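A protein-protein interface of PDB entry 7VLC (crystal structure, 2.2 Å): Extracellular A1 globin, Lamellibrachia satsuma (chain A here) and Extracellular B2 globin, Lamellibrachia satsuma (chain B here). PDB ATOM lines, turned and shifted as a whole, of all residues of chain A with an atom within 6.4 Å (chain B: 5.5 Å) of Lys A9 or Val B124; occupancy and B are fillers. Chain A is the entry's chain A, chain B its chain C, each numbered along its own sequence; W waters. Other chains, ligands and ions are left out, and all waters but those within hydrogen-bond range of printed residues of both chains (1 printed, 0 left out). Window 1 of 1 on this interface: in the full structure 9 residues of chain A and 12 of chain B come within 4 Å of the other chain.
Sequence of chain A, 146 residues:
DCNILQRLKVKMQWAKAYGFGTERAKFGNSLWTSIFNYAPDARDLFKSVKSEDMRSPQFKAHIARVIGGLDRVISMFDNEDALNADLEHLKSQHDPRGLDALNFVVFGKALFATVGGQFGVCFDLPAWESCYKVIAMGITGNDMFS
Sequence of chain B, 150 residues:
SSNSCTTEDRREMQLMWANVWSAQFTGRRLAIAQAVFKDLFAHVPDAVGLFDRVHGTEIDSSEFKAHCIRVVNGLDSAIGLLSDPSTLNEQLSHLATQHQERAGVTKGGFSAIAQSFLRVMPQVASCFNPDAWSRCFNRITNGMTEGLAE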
ATOM      1  N   ILE A   4      21.384  11.829 -14.559  1.00  0.00           N
ATOM      2  CA  ILE A   4      21.533  12.523 -15.833  1.00  0.00           C
ATOM      3  C   ILE A   4      21.467  14.037 -15.641  1.00  0.00           C
ATOM      4  O   ILE A   4      22.143  14.788 -16.355  1.00  0.00           O
ATOM      5  CB  ILE A   4      20.479  12.019 -16.839  1.00  0.00           C
ATOM      6  CG1 ILE A   4      20.693  12.659 -18.212  1.00  0.00           C
ATOM      7  CG2 ILE A   4      19.075  12.284 -16.333  1.00  0.00           C
ATOM      8  CD1 ILE A   4      19.813  12.079 -19.303  1.00  0.00           C
ATOM      9  N   LEU A   5      20.690  14.511 -14.664  1.00  0.00           N
ATOM     10  CA  LEU A   5      20.615  15.947 -14.417  1.00  0.00           C
ATOM     11  C   LEU A   5      21.931  16.482 -13.868  1.00  0.00           C
ATOM     12  O   LEU A   5      22.398  17.546 -14.289  1.00  0.00           O
ATOM     13  CB  LEU A   5      19.461  16.257 -13.459  1.00  0.00           C
ATOM     14  CG  LEU A   5      18.059  15.960 -13.991  1.00  0.00           C
ATOM     15  CD1 LEU A   5      17.003  16.521 -13.056  1.00  0.00           C
ATOM     16  CD2 LEU A   5      17.875  16.505 -15.397  1.00  0.00           C
ATOM     17  N   GLN A   6      22.548  15.753 -12.935  1.00  0.00           N
ATOM     18  CA  GLN A   6      23.845  16.167 -12.412  1.00  0.00           C
ATOM     19  C   GLN A   6      24.930  16.100 -13.481  1.00  0.00           C
ATOM     20  O   GLN A   6      25.832  16.946 -13.495  1.00  0.00           O
ATOM     21  CB  GLN A   6      24.213  15.307 -11.205  1.00  0.00           C
ATOM     22  CG  GLN A   6      23.240  15.456 -10.042  1.00  0.00           C
ATOM     23  CD  GLN A   6      23.578  14.561  -8.869  1.00  0.00           C
ATOM     24  OE1 GLN A   6      23.720  13.349  -9.021  1.00  0.00           O
ATOM     25  NE2 GLN A   6      23.707  15.155  -7.686  1.00  0.00           N
ATOM     26  N   ARG A   7      24.858  15.116 -14.386  1.00  0.00           N
ATOM     27  CA  ARG A   7      25.839  15.029 -15.465  1.00  0.00           C
ATOM     28  C   ARG A   7      25.772  16.257 -16.368  1.00  0.00           C
ATOM     29  O   ARG A   7      26.808  16.817 -16.743  1.00  0.00           O
ATOM     30  CB  ARG A   7      25.627  13.747 -16.274  1.00  0.00           C
ATOM     31  CG  ARG A   7      26.063  12.483 -15.543  1.00  0.00           C
ATOM     32  CD  ARG A   7      25.435  11.219 -16.119  1.00  0.00           C
ATOM     33  NE  ARG A   7      25.678  10.063 -15.255  1.00  0.00           N
ATOM     34  CZ  ARG A   7      26.605   9.135 -15.478  1.00  0.00           C
ATOM     35  NH1 ARG A   7      27.384   9.207 -16.549  1.00  0.00           N
ATOM     36  NH2 ARG A   7      26.750   8.132 -14.631  1.00  0.00           N
ATOM     37  N   LEU A   8      24.557  16.697 -16.718  1.00  0.00           N
ATOM     38  CA  LEU A   8      24.405  17.928 -17.492  1.00  0.00           C
ATOM     39  C   LEU A   8      24.877  19.139 -16.699  1.00  0.00           C
ATOM     40  O   LEU A   8      25.540  20.027 -17.245  1.00  0.00           O
ATOM     41  CB  LEU A   8      22.949  18.107 -17.910  1.00  0.00           C
ATOM     42  CG  LEU A   8      22.358  17.036 -18.823  1.00  0.00           C
ATOM     43  CD1 LEU A   8      20.906  17.363 -19.131  1.00  0.00           C
ATOM     44  CD2 LEU A   8      23.178  16.910 -20.103  1.00  0.00           C
ATOM     45  N   LYS A   9      24.529  19.197 -15.413  1.00  0.00           N
ATOM     46  CA  LYS A   9      25.011  20.270 -14.550  1.00  0.00           C
ATOM     47  C   LYS A   9      26.536  20.321 -14.544  1.00  0.00           C
ATOM     48  O   LYS A   9      27.134  21.393 -14.690  1.00  0.00           O
ATOM     49  CB  LYS A   9      24.463  20.068 -13.136  1.00  0.00           C
ATOM     50  CG  LYS A   9      24.765  21.189 -12.163  1.00  0.00           C
ATOM     51  CD  LYS A   9      23.919  22.400 -12.469  1.00  0.00           C
ATOM     52  CE  LYS A   9      23.760  23.276 -11.253  1.00  0.00           C
ATOM     53  NZ  LYS A   9      22.955  22.627 -10.183  1.00  0.00           N
ATOM     54  N   VAL A  10      27.183  19.159 -14.391  1.00  0.00           N
ATOM     55  CA  VAL A  10      28.643  19.106 -14.373  1.00  0.00           C
ATOM     56  C   VAL A  10      29.217  19.531 -15.720  1.00  0.00           C
ATOM     57  O   VAL A  10      30.201  20.278 -15.776  1.00  0.00           O
ATOM     58  CB  VAL A  10      29.123  17.700 -13.965  1.00  0.00           C
ATOM     59  CG1 VAL A  10      30.615  17.522 -14.251  1.00  0.00           C
ATOM     60  CG2 VAL A  10      28.838  17.462 -12.494  1.00  0.00           C
ATOM     61  N   LYS A  11      28.616  19.072 -16.826  1.00  0.00           N
ATOM     62  CA  LYS A  11      29.084  19.503 -18.142  1.00  0.00           C
ATOM     63  C   LYS A  11      28.953  21.014 -18.305  1.00  0.00           C
ATOM     64  O   LYS A  11      29.828  21.657 -18.893  1.00  0.00           O
ATOM     65  CB  LYS A  11      28.310  18.787 -19.251  1.00  0.00           C
ATOM     66  CG  LYS A  11      28.583  17.293 -19.348  1.00  0.00           C
ATOM     67  CD  LYS A  11      27.907  16.666 -20.569  1.00  0.00           C
ATOM     68  CE  LYS A  11      28.487  17.212 -21.861  1.00  0.00           C
ATOM     69  NZ  LYS A  11      27.954  16.504 -23.056  1.00  0.00           N
ATOM     70  N   MET A  12      27.860  21.589 -17.796  1.00  0.00           N
ATOM     71  CA  MET A  12      27.656  23.035 -17.857  1.00  0.00           C
ATOM     72  C   MET A  12      28.758  23.777 -17.114  1.00  0.00           C
ATOM     73  O   MET A  12      29.470  24.606 -17.689  1.00  0.00           O
ATOM     74  CB  MET A  12      26.293  23.395 -17.261  1.00  0.00           C
ATOM     75  CG  MET A  12      25.114  23.094 -18.152  1.00  0.00           C
ATOM     76  SD  MET A  12      25.185  24.079 -19.653  1.00  0.00           S
ATOM     77  CE  MET A  12      23.470  24.050 -20.143  1.00  0.00           C
ATOM     78  N   GLN A  13      28.904  23.496 -15.819  1.00  0.00           N
ATOM     79  CA  GLN A  13      29.859  24.249 -15.018  1.00  0.00           C
ATOM     80  C   GLN A  13      31.295  23.978 -15.450  1.00  0.00           C
ATOM     81  O   GLN A  13      32.144  24.869 -15.351  1.00  0.00           O
ATOM     82  CB  GLN A  13      29.657  23.922 -13.542  1.00  0.00           C
ATOM     83  CG  GLN A  13      28.235  24.180 -13.063  1.00  0.00           C
ATOM     84  CD  GLN A  13      28.091  24.021 -11.566  1.00  0.00           C
ATOM     85  OE1 GLN A  13      28.942  23.420 -10.913  1.00  0.00           O
ATOM     86  NE2 GLN A  13      27.008  24.560 -11.011  1.00  0.00           N
ATOM     87  N   TRP A  14      31.584  22.770 -15.944  1.00  0.00           N
ATOM     88  CA  TRP A  14      32.928  22.480 -16.433  1.00  0.00           C
ATOM     89  C   TRP A  14      33.276  23.357 -17.628  1.00  0.00           C
ATOM     90  O   TRP A  14      34.348  23.967 -17.668  1.00  0.00           O
ATOM     91  CB  TRP A  14      33.060  21.003 -16.809  1.00  0.00           C
ATOM     92  CG  TRP A  14      34.280  20.735 -17.638  1.00  0.00           C
ATOM     93  CD1 TRP A  14      34.334  20.552 -18.991  1.00  0.00           C
ATOM     94  CD2 TRP A  14      35.631  20.649 -17.170  1.00  0.00           C
ATOM     95  NE1 TRP A  14      35.630  20.347 -19.392  1.00  0.00           N
ATOM     96  CE2 TRP A  14      36.446  20.401 -18.292  1.00  0.00           C
ATOM     97  CE3 TRP A  14      36.227  20.747 -15.910  1.00  0.00           C
ATOM     98  CZ2 TRP A  14      37.823  20.250 -18.192  1.00  0.00           C
ATOM     99  CZ3 TRP A  14      37.591  20.601 -15.811  1.00  0.00           C
ATOM    100  CH2 TRP A  14      38.378  20.352 -16.945  1.00  0.00           C
ATOM    101  N   CYS A 122      27.630  29.580  -7.493  1.00  0.00           N
ATOM    102  CA  CYS A 122      26.623  28.631  -7.951  1.00  0.00           C
ATOM    103  C   CYS A 122      27.204  27.246  -8.232  1.00  0.00           C
ATOM    104  O   CYS A 122      26.501  26.382  -8.769  1.00  0.00           O
ATOM    105  CB  CYS A 122      25.915  29.182  -9.191  1.00  0.00           C
ATOM    106  SG  CYS A 122      25.209  30.846  -8.934  1.00  0.00           S
ATOM    107  N   PHE A 123      28.466  27.027  -7.877  1.00  0.00           N
ATOM    108  CA  PHE A 123      29.083  25.717  -8.009  1.00  0.00           C
ATOM    109  C   PHE A 123      28.270  24.675  -7.249  1.00  0.00           C
ATOM    110  O   PHE A 123      27.932  24.865  -6.076  1.00  0.00           O
ATOM    111  CB  PHE A 123      30.516  25.793  -7.481  1.00  0.00           C
ATOM    112  CG  PHE A 123      31.265  24.491  -7.515  1.00  0.00           C
ATOM    113  CD1 PHE A 123      31.610  23.906  -8.722  1.00  0.00           C
ATOM    114  CD2 PHE A 123      31.675  23.883  -6.339  1.00  0.00           C
ATOM    115  CE1 PHE A 123      32.323  22.720  -8.760  1.00  0.00           C
ATOM    116  CE2 PHE A 123      32.392  22.694  -6.369  1.00  0.00           C
ATOM    117  CZ  PHE A 123      32.713  22.112  -7.585  1.00  0.00           C
ATOM    118  N   ASP A 124      27.926  23.582  -7.938  1.00  0.00           N
ATOM    119  CA  ASP A 124      27.136  22.498  -7.351  1.00  0.00           C
ATOM    120  C   ASP A 124      28.103  21.440  -6.840  1.00  0.00           C
ATOM    121  O   ASP A 124      28.443  20.485  -7.540  1.00  0.00           O
ATOM    122  CB  ASP A 124      26.159  21.924  -8.376  1.00  0.00           C
ATOM    123  CG  ASP A 124      25.106  21.012  -7.750  1.00  0.00           C
ATOM    124  OD1 ASP A 124      25.385  20.363  -6.711  1.00  0.00           O
ATOM    125  OD2 ASP A 124      23.999  20.941  -8.315  1.00  0.00           O
ATOM    126  N   ALA A 127      26.873  17.626  -6.755  1.00  0.00           N
ATOM    127  CA  ALA A 127      26.869  17.024  -8.083  1.00  0.00           C
ATOM    128  C   ALA A 127      28.279  16.656  -8.530  1.00  0.00           C
ATOM    129  O   ALA A 127      28.489  15.592  -9.126  1.00  0.00           O
ATOM    130  CB  ALA A 127      26.217  17.975  -9.083  1.00  0.00           C
ATOM    131  N   TRP A 128      29.262  17.518  -8.242  1.00  0.00           N
ATOM    132  CA  TRP A 128      30.635  17.234  -8.646  1.00  0.00           C
ATOM    133  C   TRP A 128      31.237  16.090  -7.833  1.00  0.00           C
ATOM    134  O   TRP A 128      31.985  15.270  -8.374  1.00  0.00           O
ATOM    135  CB  TRP A 128      31.485  18.495  -8.528  1.00  0.00           C
ATOM    136  CG  TRP A 128      31.334  19.416  -9.700  1.00  0.00           C
ATOM    137  CD1 TRP A 128      30.361  20.358  -9.887  1.00  0.00           C
ATOM    138  CD2 TRP A 128      32.174  19.472 -10.856  1.00  0.00           C
ATOM    139  NE1 TRP A 128      30.548  21.002 -11.084  1.00  0.00           N
ATOM    140  CE2 TRP A 128      31.656  20.477 -11.698  1.00  0.00           C
ATOM    141  CE3 TRP A 128      33.316  18.772 -11.261  1.00  0.00           C
ATOM    142  CZ2 TRP A 128      32.235  20.795 -12.919  1.00  0.00           C
ATOM    143  CZ3 TRP A 128      33.892  19.093 -12.470  1.00  0.00           C
ATOM    144  CH2 TRP A 128      33.349  20.098 -13.288  1.00  0.00           C
ATOM    145  N   ASN B  19      20.658  29.322 -19.397  1.00  0.00           N
ATOM    146  CA  ASN B  19      21.830  28.633 -18.869  1.00  0.00           C
ATOM    147  C   ASN B  19      21.624  27.143 -18.747  1.00  0.00           C
ATOM    148  O   ASN B  19      22.501  26.466 -18.188  1.00  0.00           O
ATOM    149  CB  ASN B  19      22.221  29.213 -17.507  1.00  0.00           C
ATOM    150  CG  ASN B  19      22.954  30.543 -17.624  1.00  0.00           C
ATOM    151  OD1 ASN B  19      22.368  31.553 -18.013  1.00  0.00           O
ATOM    152  ND2 ASN B  19      24.240  30.548 -17.278  1.00  0.00           N
ATOM    153  N   VAL B  20      20.503  26.611 -19.236  1.00  0.00           N
ATOM    154  CA  VAL B  20      20.242  25.177 -19.201  1.00  0.00           C
ATOM    155  C   VAL B  20      19.779  24.716 -20.575  1.00  0.00           C
ATOM    156  O   VAL B  20      19.996  23.565 -20.968  1.00  0.00           O
ATOM    157  CB  VAL B  20      19.198  24.825 -18.130  1.00  0.00           C
ATOM    158  CG1 VAL B  20      19.195  23.341 -17.890  1.00  0.00           C
ATOM    159  CG2 VAL B  20      19.498  25.558 -16.852  1.00  0.00           C
ATOM    160  N   ILE B  32      15.574  17.194 -19.296  1.00  0.00           N
ATOM    161  CA  ILE B  32      14.775  17.993 -18.373  1.00  0.00           C
ATOM    162  C   ILE B  32      13.307  17.590 -18.440  1.00  0.00           C
ATOM    163  O   ILE B  32      12.642  17.451 -17.407  1.00  0.00           O
ATOM    164  CB  ILE B  32      14.956  19.492 -18.672  1.00  0.00           C
ATOM    165  CG1 ILE B  32      16.417  19.900 -18.491  1.00  0.00           C
ATOM    166  CG2 ILE B  32      14.051  20.322 -17.775  1.00  0.00           C
ATOM    167  CD1 ILE B  32      16.738  21.219 -19.142  1.00  0.00           C
ATOM    168  N   VAL B 120      13.179  19.535 -10.399  1.00  0.00           N
ATOM    169  CA  VAL B 120      14.107  19.215 -11.477  1.00  0.00           C
ATOM    170  C   VAL B 120      15.087  20.361 -11.722  1.00  0.00           C
ATOM    171  O   VAL B 120      16.293  20.138 -11.873  1.00  0.00           O
ATOM    172  CB  VAL B 120      13.318  18.863 -12.750  1.00  0.00           C
ATOM    173  CG1 VAL B 120      14.236  18.810 -13.954  1.00  0.00           C
ATOM    174  CG2 VAL B 120      12.585  17.542 -12.576  1.00  0.00           C
ATOM    175  N   MET B 121      14.590  21.600 -11.753  1.00  0.00           N
ATOM    176  CA  MET B 121      15.407  22.727 -12.205  1.00  0.00           C
ATOM    177  C   MET B 121      16.662  22.965 -11.370  1.00  0.00           C
ATOM    178  O   MET B 121      17.734  23.174 -11.965  1.00  0.00           O
ATOM    179  CB  MET B 121      14.539  23.986 -12.272  1.00  0.00           C
ATOM    180  CG  MET B 121      13.578  23.996 -13.443  1.00  0.00           C
ATOM    181  SD  MET B 121      14.426  23.949 -15.032  1.00  0.00           S
ATOM    182  CE  MET B 121      15.449  25.413 -14.910  1.00  0.00           C
ATOM    183  N   PRO B 122      16.623  22.964 -10.034  1.00  0.00           N
ATOM    184  CA  PRO B 122      17.868  23.188  -9.280  1.00  0.00           C
ATOM    185  C   PRO B 122      18.921  22.108  -9.489  1.00  0.00           C
ATOM    186  O   PRO B 122      20.106  22.377  -9.260  1.00  0.00           O
ATOM    187  CB  PRO B 122      17.394  23.239  -7.819  1.00  0.00           C
ATOM    188  CG  PRO B 122      16.096  22.515  -7.812  1.00  0.00           C
ATOM    189  CD  PRO B 122      15.465  22.825  -9.130  1.00  0.00           C
ATOM    190  N   GLN B 123      18.535  20.904  -9.921  1.00  0.00           N
ATOM    191  CA  GLN B 123      19.517  19.858 -10.192  1.00  0.00           C
ATOM    192  C   GLN B 123      20.296  20.116 -11.473  1.00  0.00           C
ATOM    193  O   GLN B 123      21.412  19.607 -11.625  1.00  0.00           O
ATOM    194  CB  GLN B 123      18.839  18.493 -10.296  1.00  0.00           C
ATOM    195  CG  GLN B 123      18.238  17.969  -9.010  1.00  0.00           C
ATOM    196  CD  GLN B 123      17.518  16.656  -9.227  1.00  0.00           C
ATOM    197  OE1 GLN B 123      18.119  15.669  -9.649  1.00  0.00           O
ATOM    198  NE2 GLN B 123      16.219  16.645  -8.964  1.00  0.00           N
ATOM    199  N   VAL B 124      19.736  20.886 -12.397  1.00  0.00           N
ATOM    200  CA  VAL B 124      20.373  21.107 -13.684  1.00  0.00           C
ATOM    201  C   VAL B 124      20.733  22.567 -13.928  1.00  0.00           C
ATOM    202  O   VAL B 124      21.643  22.836 -14.729  1.00  0.00           O
ATOM    203  CB  VAL B 124      19.481  20.569 -14.825  1.00  0.00           C
ATOM    204  CG1 VAL B 124      18.270  21.461 -15.020  1.00  0.00           C
ATOM    205  CG2 VAL B 124      20.274  20.393 -16.116  1.00  0.00           C
ATOM    206  N   ALA B 125      20.085  23.514 -13.251  1.00  0.00           N
ATOM    207  CA  ALA B 125      20.316  24.939 -13.442  1.00  0.00           C
ATOM    208  C   ALA B 125      21.251  25.481 -12.373  1.00  0.00           C
ATOM    209  O   ALA B 125      21.116  25.156 -11.190  1.00  0.00           O
ATOM    210  CB  ALA B 125      19.001  25.722 -13.398  1.00  0.00           C
ATOM    211  N   SER B 126      22.189  26.321 -12.796  1.00  0.00           N
ATOM    212  CA  SER B 126      23.056  27.044 -11.877  1.00  0.00           C
ATOM    213  C   SER B 126      22.435  28.391 -11.529  1.00  0.00           C
ATOM    214  O   SER B 126      21.802  29.029 -12.373  1.00  0.00           O
ATOM    215  CB  SER B 126      24.442  27.248 -12.490  1.00  0.00           C
ATOM    216  OG  SER B 126      25.028  26.009 -12.844  1.00  0.00           O
HETATM  217  O   HOH W   1      22.694  18.876  -9.522  1.00  0.00           O
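NZ of Lys A9 is in hydrogen-bond range of O of Pro B122 (3.0 Å). NZ of Lys A9 lies close to O of Ala B125, 3.3 Å away. NE2 of Gln A13 sits at hydrogen-bond distance from OG of Ser B126 (3.1 Å).
OD2 of Asp A124 is in salt-bridge range of NZ of Lys A9 (2.7 Å). O of Cys A122 sits at hydrogen-bond distance from NE2 of Gln A13 (2.9 Å). The backbone NH (N) of Asp A124 lies within hydrogen-bond range of the side-chain amide oxygen (OE1) of Gln A13, at 3.1 Å. The indole nitrogen of Trp A128 sits at hydrogen-bond distance from the side-chain amide oxygen of Gln A13 (2.9 Å).
Leu A5 touches Val B120. Gln B123 touches Leu A5. Val B124 touches Leu A5 (CG2 to O, 3.99 Å). CB of Leu A8 touches CG2 of Val B124, at 3.9 Å. Gln B123 touches Lys A9. Val B124 touches Lys A9. CE of Lys A9 touches OG of Ser B126 (3.4 Å). Met A12 touches Asn B19. CE of Met A12 touches CA of Val B20, at 3.5 Å.
Lys A9 touches just these residues of chain B: Pro B122 (3.0 Å), Gln B123 (3.4 Å), Val B124 (3.2 Å), Ala B125 (3.2 Å) and Ser B126 (3.4 Å). Of the printed residues of chain A, Val B124 touches Leu A5, Leu A8 and Lys A9. Of the printed residues of chain A, Val B20 touches Met A12 (3.5 Å). Printed residues of chain B within 4 Å of Met A12: Asn B19 (3.3 Å) and Val B20 (3.5 Å). Of the printed residues of chain A, Ala B125 touches Lys A9. Of the printed residues of chain B, Leu A5 touches Val B120, Gln B123 and Val B124. Of the printed residues of chain B, Leu A8 touches Val B124. The nearest printed residue of chain A that does not touch Val B124 is Met A12 (4.9 Å). The nearest printed residue of chain A that does not touch Val B20 is Leu A8 (6.3 Å).
Of the 10 printed residues of chain B, 8 touch a printed residue of chain A. Printed residues of chain B that touch a printed residue of chain A: Asn B19, Val B20, Val B120, Pro B122, Gln B123, Val B124, Ala B125 and Ser B126. Hydrophobic or aromatic side chains of chain B within 4 Å of the printed part of chain A: Val B120 and Val B124. Of the 16 printed residues of chain A, 5 touch a printed residue of chain B. Hydrophobic or aromatic side chains of chain A within 4 Å of the printed part of chain B: Leu A5, Leu A8 and Met A12. Among the printed residues, 12 pairs touch across the chains. Among the printed residues, no Asp or Glu carboxylate lies within 4 Å of a Lys or Arg side-chain nitrogen of the other chain.
Water W1 bridges the backbone carbonyl oxygen of Gln B123 and the side-chain carboxylate of Asp A124.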
